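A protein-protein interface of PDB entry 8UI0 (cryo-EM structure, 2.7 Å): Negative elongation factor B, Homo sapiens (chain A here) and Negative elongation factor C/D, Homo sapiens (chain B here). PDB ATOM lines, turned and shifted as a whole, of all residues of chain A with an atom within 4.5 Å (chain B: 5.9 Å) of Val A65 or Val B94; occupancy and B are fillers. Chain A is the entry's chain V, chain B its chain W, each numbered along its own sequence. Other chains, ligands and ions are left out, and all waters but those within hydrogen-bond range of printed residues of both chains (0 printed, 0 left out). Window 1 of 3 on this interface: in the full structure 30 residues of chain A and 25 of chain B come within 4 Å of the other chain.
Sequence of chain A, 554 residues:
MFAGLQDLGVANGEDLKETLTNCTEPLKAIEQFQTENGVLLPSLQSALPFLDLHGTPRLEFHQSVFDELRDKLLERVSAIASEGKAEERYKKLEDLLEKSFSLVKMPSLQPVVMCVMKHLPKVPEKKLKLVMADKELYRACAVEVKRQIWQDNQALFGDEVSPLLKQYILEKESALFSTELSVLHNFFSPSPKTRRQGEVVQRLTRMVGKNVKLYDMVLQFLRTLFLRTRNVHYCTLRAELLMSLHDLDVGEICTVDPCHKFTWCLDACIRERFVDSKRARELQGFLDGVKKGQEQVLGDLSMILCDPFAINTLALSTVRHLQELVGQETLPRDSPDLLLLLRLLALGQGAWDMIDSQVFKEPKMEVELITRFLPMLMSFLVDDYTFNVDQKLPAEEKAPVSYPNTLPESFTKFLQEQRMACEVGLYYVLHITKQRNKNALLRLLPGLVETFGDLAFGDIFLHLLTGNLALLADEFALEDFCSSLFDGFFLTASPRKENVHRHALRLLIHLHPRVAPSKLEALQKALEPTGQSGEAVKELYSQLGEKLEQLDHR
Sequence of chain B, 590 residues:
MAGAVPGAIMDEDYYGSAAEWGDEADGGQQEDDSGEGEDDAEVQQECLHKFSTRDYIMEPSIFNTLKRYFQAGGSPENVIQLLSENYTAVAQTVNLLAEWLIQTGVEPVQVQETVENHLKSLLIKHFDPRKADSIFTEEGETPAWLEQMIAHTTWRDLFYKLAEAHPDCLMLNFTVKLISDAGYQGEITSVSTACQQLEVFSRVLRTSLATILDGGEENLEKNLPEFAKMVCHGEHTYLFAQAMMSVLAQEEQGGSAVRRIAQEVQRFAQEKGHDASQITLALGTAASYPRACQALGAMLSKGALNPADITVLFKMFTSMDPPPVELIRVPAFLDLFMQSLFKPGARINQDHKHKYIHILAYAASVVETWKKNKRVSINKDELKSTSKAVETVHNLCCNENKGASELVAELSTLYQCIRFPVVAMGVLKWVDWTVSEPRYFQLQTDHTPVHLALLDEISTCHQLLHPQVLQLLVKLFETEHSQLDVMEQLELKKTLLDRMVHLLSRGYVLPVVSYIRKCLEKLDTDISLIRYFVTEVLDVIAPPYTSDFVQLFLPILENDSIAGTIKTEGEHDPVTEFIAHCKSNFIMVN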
ATOM      1  N   VAL A  39     -26.642 -21.503 -18.927  1.00  0.00           N
ATOM      2  CA  VAL A  39     -26.328 -21.220 -20.323  1.00  0.00           C
ATOM      3  C   VAL A  39     -25.518 -22.404 -20.838  1.00  0.00           C
ATOM      4  O   VAL A  39     -24.491 -22.767 -20.256  1.00  0.00           O
ATOM      5  CB  VAL A  39     -25.566 -19.894 -20.472  1.00  0.00           C
ATOM      6  CG1 VAL A  39     -25.410 -19.495 -21.945  1.00  0.00           C
ATOM      7  CG2 VAL A  39     -26.282 -18.779 -19.718  1.00  0.00           C
ATOM      8  N   PHE A  61     -22.155 -11.821 -15.434  1.00  0.00           N
ATOM      9  CA  PHE A  61     -21.805 -11.986 -16.838  1.00  0.00           C
ATOM     10  C   PHE A  61     -23.042 -12.357 -17.643  1.00  0.00           C
ATOM     11  O   PHE A  61     -23.135 -12.007 -18.829  1.00  0.00           O
ATOM     12  CB  PHE A  61     -20.662 -13.006 -17.016  1.00  0.00           C
ATOM     13  CG  PHE A  61     -21.086 -14.460 -17.035  1.00  0.00           C
ATOM     14  CD1 PHE A  61     -21.402 -15.099 -18.230  1.00  0.00           C
ATOM     15  CD2 PHE A  61     -21.107 -15.203 -15.870  1.00  0.00           C
ATOM     16  CE1 PHE A  61     -21.774 -16.429 -18.248  1.00  0.00           C
ATOM     17  CE2 PHE A  61     -21.479 -16.537 -15.888  1.00  0.00           C
ATOM     18  CZ  PHE A  61     -21.808 -17.148 -17.077  1.00  0.00           C
ATOM     19  N   HIS A  62     -24.022 -13.025 -17.014  1.00  0.00           N
ATOM     20  CA  HIS A  62     -25.294 -13.207 -17.704  1.00  0.00           C
ATOM     21  C   HIS A  62     -25.956 -11.863 -18.018  1.00  0.00           C
ATOM     22  O   HIS A  62     -26.525 -11.690 -19.090  1.00  0.00           O
ATOM     23  CB  HIS A  62     -26.250 -14.081 -16.895  1.00  0.00           C
ATOM     24  CG  HIS A  62     -25.788 -15.495 -16.716  1.00  0.00           C
ATOM     25  ND1 HIS A  62     -25.945 -16.182 -15.531  1.00  0.00           N
ATOM     26  CD2 HIS A  62     -25.178 -16.352 -17.568  1.00  0.00           C
ATOM     27  CE1 HIS A  62     -25.453 -17.401 -15.663  1.00  0.00           C
ATOM     28  NE2 HIS A  62     -24.979 -17.528 -16.888  1.00  0.00           N
ATOM     29  N   GLN A  63     -25.896 -10.899 -17.100  1.00  0.00           N
ATOM     30  CA  GLN A  63     -26.507  -9.596 -17.359  1.00  0.00           C
ATOM     31  C   GLN A  63     -25.804  -8.881 -18.507  1.00  0.00           C
ATOM     32  O   GLN A  63     -26.458  -8.277 -19.377  1.00  0.00           O
ATOM     33  CB  GLN A  63     -26.478  -8.746 -16.085  1.00  0.00           C
ATOM     34  CG  GLN A  63     -26.629  -7.234 -16.302  1.00  0.00           C
ATOM     35  CD  GLN A  63     -26.959  -6.477 -15.028  1.00  0.00           C
ATOM     36  OE1 GLN A  63     -27.160  -7.070 -13.968  1.00  0.00           O
ATOM     37  NE2 GLN A  63     -27.011  -5.154 -15.129  1.00  0.00           N
ATOM     38  N   SER A  64     -24.470  -8.935 -18.520  1.00  0.00           N
ATOM     39  CA  SER A  64     -23.716  -8.294 -19.596  1.00  0.00           C
ATOM     40  C   SER A  64     -24.071  -8.900 -20.952  1.00  0.00           C
ATOM     41  O   SER A  64     -24.422  -8.180 -21.904  1.00  0.00           O
ATOM     42  CB  SER A  64     -22.214  -8.416 -19.326  1.00  0.00           C
ATOM     43  OG  SER A  64     -21.765  -9.742 -19.536  1.00  0.00           O
ATOM     44  N   VAL A  65     -24.018 -10.231 -21.053  1.00  0.00           N
ATOM     45  CA  VAL A  65     -24.358 -10.862 -22.323  1.00  0.00           C
ATOM     46  C   VAL A  65     -25.847 -10.708 -22.622  1.00  0.00           C
ATOM     47  O   VAL A  65     -26.244 -10.704 -23.783  1.00  0.00           O
ATOM     48  CB  VAL A  65     -23.916 -12.342 -22.354  1.00  0.00           C
ATOM     49  CG1 VAL A  65     -22.427 -12.469 -22.038  1.00  0.00           C
ATOM     50  CG2 VAL A  65     -24.741 -13.193 -21.414  1.00  0.00           C
ATOM     51  N   PHE A  66     -26.692 -10.559 -21.600  1.00  0.00           N
ATOM     52  CA  PHE A  66     -28.115 -10.311 -21.827  1.00  0.00           C
ATOM     53  C   PHE A  66     -28.321  -9.005 -22.581  1.00  0.00           C
ATOM     54  O   PHE A  66     -29.022  -8.962 -23.603  1.00  0.00           O
ATOM     55  CB  PHE A  66     -28.850 -10.309 -20.474  1.00  0.00           C
ATOM     56  CG  PHE A  66     -30.069  -9.420 -20.414  1.00  0.00           C
ATOM     57  CD1 PHE A  66     -31.306  -9.892 -20.809  1.00  0.00           C
ATOM     58  CD2 PHE A  66     -29.987  -8.136 -19.889  1.00  0.00           C
ATOM     59  CE1 PHE A  66     -32.428  -9.086 -20.741  1.00  0.00           C
ATOM     60  CE2 PHE A  66     -31.105  -7.328 -19.818  1.00  0.00           C
ATOM     61  CZ  PHE A  66     -32.328  -7.805 -20.241  1.00  0.00           C
ATOM     62  N   ASP A  67     -27.682  -7.933 -22.103  1.00  0.00           N
ATOM     63  CA  ASP A  67     -27.772  -6.652 -22.799  1.00  0.00           C
ATOM     64  C   ASP A  67     -27.227  -6.766 -24.220  1.00  0.00           C
ATOM     65  O   ASP A  67     -27.891  -6.363 -25.189  1.00  0.00           O
ATOM     66  CB  ASP A  67     -27.019  -5.576 -22.016  1.00  0.00           C
ATOM     67  CG  ASP A  67     -27.571  -4.185 -22.259  1.00  0.00           C
ATOM     68  OD1 ASP A  67     -28.091  -3.935 -23.367  1.00  0.00           O
ATOM     69  OD2 ASP A  67     -27.490  -3.342 -21.341  1.00  0.00           O
ATOM     70  N   GLU A  68     -26.041  -7.376 -24.364  1.00  0.00           N
ATOM     71  CA  GLU A  68     -25.405  -7.492 -25.678  1.00  0.00           C
ATOM     72  C   GLU A  68     -26.277  -8.280 -26.657  1.00  0.00           C
ATOM     73  O   GLU A  68     -26.526  -7.841 -27.792  1.00  0.00           O
ATOM     74  CB  GLU A  68     -24.038  -8.163 -25.517  1.00  0.00           C
ATOM     75  CG  GLU A  68     -23.151  -8.159 -26.761  1.00  0.00           C
ATOM     76  CD  GLU A  68     -22.607  -6.785 -27.096  1.00  0.00           C
ATOM     77  OE1 GLU A  68     -22.213  -6.054 -26.163  1.00  0.00           O
ATOM     78  OE2 GLU A  68     -22.570  -6.435 -28.294  1.00  0.00           O
ATOM     79  N   LEU A  69     -26.776  -9.433 -26.222  1.00  0.00           N
ATOM     80  CA  LEU A  69     -27.464 -10.340 -27.125  1.00  0.00           C
ATOM     81  C   LEU A  69     -28.866  -9.855 -27.466  1.00  0.00           C
ATOM     82  O   LEU A  69     -29.307 -10.064 -28.599  1.00  0.00           O
ATOM     83  CB  LEU A  69     -27.498 -11.752 -26.526  1.00  0.00           C
ATOM     84  CG  LEU A  69     -26.139 -12.411 -26.215  1.00  0.00           C
ATOM     85  CD1 LEU A  69     -26.299 -13.512 -25.172  1.00  0.00           C
ATOM     86  CD2 LEU A  69     -25.463 -12.969 -27.443  1.00  0.00           C
ATOM     87  N   ALA B  89     -33.703 -14.139 -12.584  1.00  0.00           N
ATOM     88  CA  ALA B  89     -33.577 -15.139 -13.645  1.00  0.00           C
ATOM     89  C   ALA B  89     -32.889 -14.534 -14.865  1.00  0.00           C
ATOM     90  O   ALA B  89     -33.352 -14.660 -16.002  1.00  0.00           O
ATOM     91  CB  ALA B  89     -34.933 -15.751 -14.013  1.00  0.00           C
ATOM     92  N   VAL B  90     -31.766 -13.861 -14.611  1.00  0.00           N
ATOM     93  CA  VAL B  90     -30.965 -13.300 -15.694  1.00  0.00           C
ATOM     94  C   VAL B  90     -30.385 -14.421 -16.550  1.00  0.00           C
ATOM     95  O   VAL B  90     -30.246 -14.274 -17.770  1.00  0.00           O
ATOM     96  CB  VAL B  90     -29.862 -12.376 -15.123  1.00  0.00           C
ATOM     97  CG1 VAL B  90     -29.058 -11.727 -16.251  1.00  0.00           C
ATOM     98  CG2 VAL B  90     -30.468 -11.301 -14.210  1.00  0.00           C
ATOM     99  N   ALA B  91     -30.044 -15.558 -15.930  1.00  0.00           N
ATOM    100  CA  ALA B  91     -29.433 -16.663 -16.664  1.00  0.00           C
ATOM    101  C   ALA B  91     -30.389 -17.261 -17.693  1.00  0.00           C
ATOM    102  O   ALA B  91     -29.992 -17.535 -18.831  1.00  0.00           O
ATOM    103  CB  ALA B  91     -28.965 -17.740 -15.686  1.00  0.00           C
ATOM    104  N   GLN B  92     -31.651 -17.478 -17.317  1.00  0.00           N
ATOM    105  CA  GLN B  92     -32.605 -18.018 -18.282  1.00  0.00           C
ATOM    106  C   GLN B  92     -32.964 -16.979 -19.338  1.00  0.00           C
ATOM    107  O   GLN B  92     -33.264 -17.334 -20.487  1.00  0.00           O
ATOM    108  CB  GLN B  92     -33.859 -18.519 -17.561  1.00  0.00           C
ATOM    109  CG  GLN B  92     -34.769 -19.416 -18.401  1.00  0.00           C
ATOM    110  CD  GLN B  92     -34.112 -20.728 -18.801  1.00  0.00           C
ATOM    111  OE1 GLN B  92     -33.551 -21.436 -17.964  1.00  0.00           O
ATOM    112  NE2 GLN B  92     -34.168 -21.052 -20.089  1.00  0.00           N
ATOM    113  N   THR B  93     -32.927 -15.697 -18.971  1.00  0.00           N
ATOM    114  CA  THR B  93     -33.031 -14.638 -19.968  1.00  0.00           C
ATOM    115  C   THR B  93     -31.908 -14.755 -20.992  1.00  0.00           C
ATOM    116  O   THR B  93     -32.134 -14.599 -22.198  1.00  0.00           O
ATOM    117  CB  THR B  93     -33.009 -13.271 -19.278  1.00  0.00           C
ATOM    118  OG1 THR B  93     -33.669 -13.360 -18.009  1.00  0.00           O
ATOM    119  CG2 THR B  93     -33.714 -12.218 -20.120  1.00  0.00           C
ATOM    120  N   VAL B  94     -30.695 -15.065 -20.531  1.00  0.00           N
ATOM    121  CA  VAL B  94     -29.578 -15.258 -21.452  1.00  0.00           C
ATOM    122  C   VAL B  94     -29.791 -16.497 -22.304  1.00  0.00           C
ATOM    123  O   VAL B  94     -29.393 -16.527 -23.470  1.00  0.00           O
ATOM    124  CB  VAL B  94     -28.250 -15.334 -20.682  1.00  0.00           C
ATOM    125  CG1 VAL B  94     -27.109 -15.864 -21.577  1.00  0.00           C
ATOM    126  CG2 VAL B  94     -27.913 -13.990 -20.167  1.00  0.00           C
ATOM    127  N   ASN B  95     -30.352 -17.558 -21.719  1.00  0.00           N
ATOM    128  CA  ASN B  95     -30.679 -18.750 -22.500  1.00  0.00           C
ATOM    129  C   ASN B  95     -31.595 -18.394 -23.664  1.00  0.00           C
ATOM    130  O   ASN B  95     -31.311 -18.725 -24.823  1.00  0.00           O
ATOM    131  CB  ASN B  95     -31.340 -19.802 -21.609  1.00  0.00           C
ATOM    132  CG  ASN B  95     -30.342 -20.612 -20.816  1.00  0.00           C
ATOM    133  OD1 ASN B  95     -30.187 -20.423 -19.609  1.00  0.00           O
ATOM    134  ND2 ASN B  95     -29.682 -21.547 -21.485  1.00  0.00           N
ATOM    135  N   LEU B  96     -32.675 -17.667 -23.365  1.00  0.00           N
ATOM    136  CA  LEU B  96     -33.619 -17.244 -24.397  1.00  0.00           C
ATOM    137  C   LEU B  96     -32.939 -16.372 -25.452  1.00  0.00           C
ATOM    138  O   LEU B  96     -33.086 -16.601 -26.659  1.00  0.00           O
ATOM    139  CB  LEU B  96     -34.781 -16.496 -23.739  1.00  0.00           C
ATOM    140  CG  LEU B  96     -35.653 -17.270 -22.744  1.00  0.00           C
ATOM    141  CD1 LEU B  96     -36.168 -16.365 -21.630  1.00  0.00           C
ATOM    142  CD2 LEU B  96     -36.821 -17.922 -23.466  1.00  0.00           C
ATOM    143  N   LEU B  97     -32.151 -15.391 -25.012  1.00  0.00           N
ATOM    144  CA  LEU B  97     -31.535 -14.451 -25.948  1.00  0.00           C
ATOM    145  C   LEU B  97     -30.480 -15.126 -26.822  1.00  0.00           C
ATOM    146  O   LEU B  97     -30.434 -14.904 -28.039  1.00  0.00           O
ATOM    147  CB  LEU B  97     -30.919 -13.291 -25.173  1.00  0.00           C
ATOM    148  CG  LEU B  97     -31.784 -12.086 -24.782  1.00  0.00           C
ATOM    149  CD1 LEU B  97     -33.149 -12.384 -24.150  1.00  0.00           C
ATOM    150  CD2 LEU B  97     -30.946 -11.285 -23.815  1.00  0.00           C
ATOM    151  N   ALA B  98     -29.603 -15.926 -26.215  1.00  0.00           N
ATOM    152  CA  ALA B  98     -28.543 -16.582 -26.971  1.00  0.00           C
ATOM    153  C   ALA B  98     -29.111 -17.603 -27.945  1.00  0.00           C
ATOM    154  O   ALA B  98     -28.675 -17.675 -29.102  1.00  0.00           O
ATOM    155  CB  ALA B  98     -27.552 -17.241 -26.013  1.00  0.00           C
ATOM    156  N   GLU B  99     -30.091 -18.404 -27.508  1.00  0.00           N
ATOM    157  CA  GLU B  99     -30.688 -19.350 -28.438  1.00  0.00           C
ATOM    158  C   GLU B  99     -31.483 -18.642 -29.527  1.00  0.00           C
ATOM    159  O   GLU B  99     -31.619 -19.193 -30.624  1.00  0.00           O
ATOM    160  CB  GLU B  99     -31.557 -20.368 -27.686  1.00  0.00           C
ATOM    161  CG  GLU B  99     -32.933 -19.888 -27.255  1.00  0.00           C
ATOM    162  CD  GLU B  99     -33.595 -20.827 -26.266  1.00  0.00           C
ATOM    163  OE1 GLU B  99     -33.130 -21.979 -26.132  1.00  0.00           O
ATOM    164  OE2 GLU B  99     -34.582 -20.414 -25.623  1.00  0.00           O
ATOM    165  N   VAL B 115     -18.266 -12.757 -25.944  1.00  0.00           N
ATOM    166  CA  VAL B 115     -18.230 -13.126 -24.532  1.00  0.00           C
ATOM    167  C   VAL B 115     -16.791 -13.239 -24.042  1.00  0.00           C
ATOM    168  O   VAL B 115     -16.459 -12.777 -22.940  1.00  0.00           O
ATOM    169  CB  VAL B 115     -19.014 -14.433 -24.301  1.00  0.00           C
ATOM    170  CG1 VAL B 115     -18.820 -14.933 -22.867  1.00  0.00           C
ATOM    171  CG2 VAL B 115     -20.492 -14.217 -24.592  1.00  0.00           C
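Among the printed residues, merely in contact across the chains: Val A39 with Val B94, Val A39 with Asn B95, His A62 with Val B90, His A62 with Ala B91, His A62 with Val B94, Gln A63 with Val B90, Val A65 with Val B94, Val A65 with Val B115, Phe A66 with Thr B93, Phe A66 with Val B94, Phe A66 with Leu B97 and Leu A69 with Leu B97.
O of Ala B89 lies within hydrogen-bond range of OG1 of Thr B93 (2.4 Å). O of Ala B91 sits close to OD1 of Asn B95, at 3.0 Å.
Hydrophobic or aromatic side chains of chain A within 4 Å of the printed part of chain B: Val A39, His A62, Val A65, Phe A66 and Leu A69. Along chain A the printed residues that touch a printed residue of chain B span positions 39 to 69. Printed residues of chain B that touch a printed residue of chain A: Val B90, Ala B91, Thr B93, Val B94, Asn B95, Leu B97 and Val B115.
Val A65 touches just these residues of chain B: Val B94 (3.5 Å) and Val B115 (3.7 Å). Of the printed residues of chain A, Leu B97 touches Phe A66 and Leu A69. Of the printed residues of chain A, Val B115 touches Val A65 (3.7 Å). Printed residues of chain A within 4 Å of Thr B93: Phe A66 (3.4 Å). The nearest residue of chain A that does not touch Val B94 is Leu A69 (4.4 Å). The nearest printed residue of chain B that does not touch Gln A63 is Val B94 (4.8 Å).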
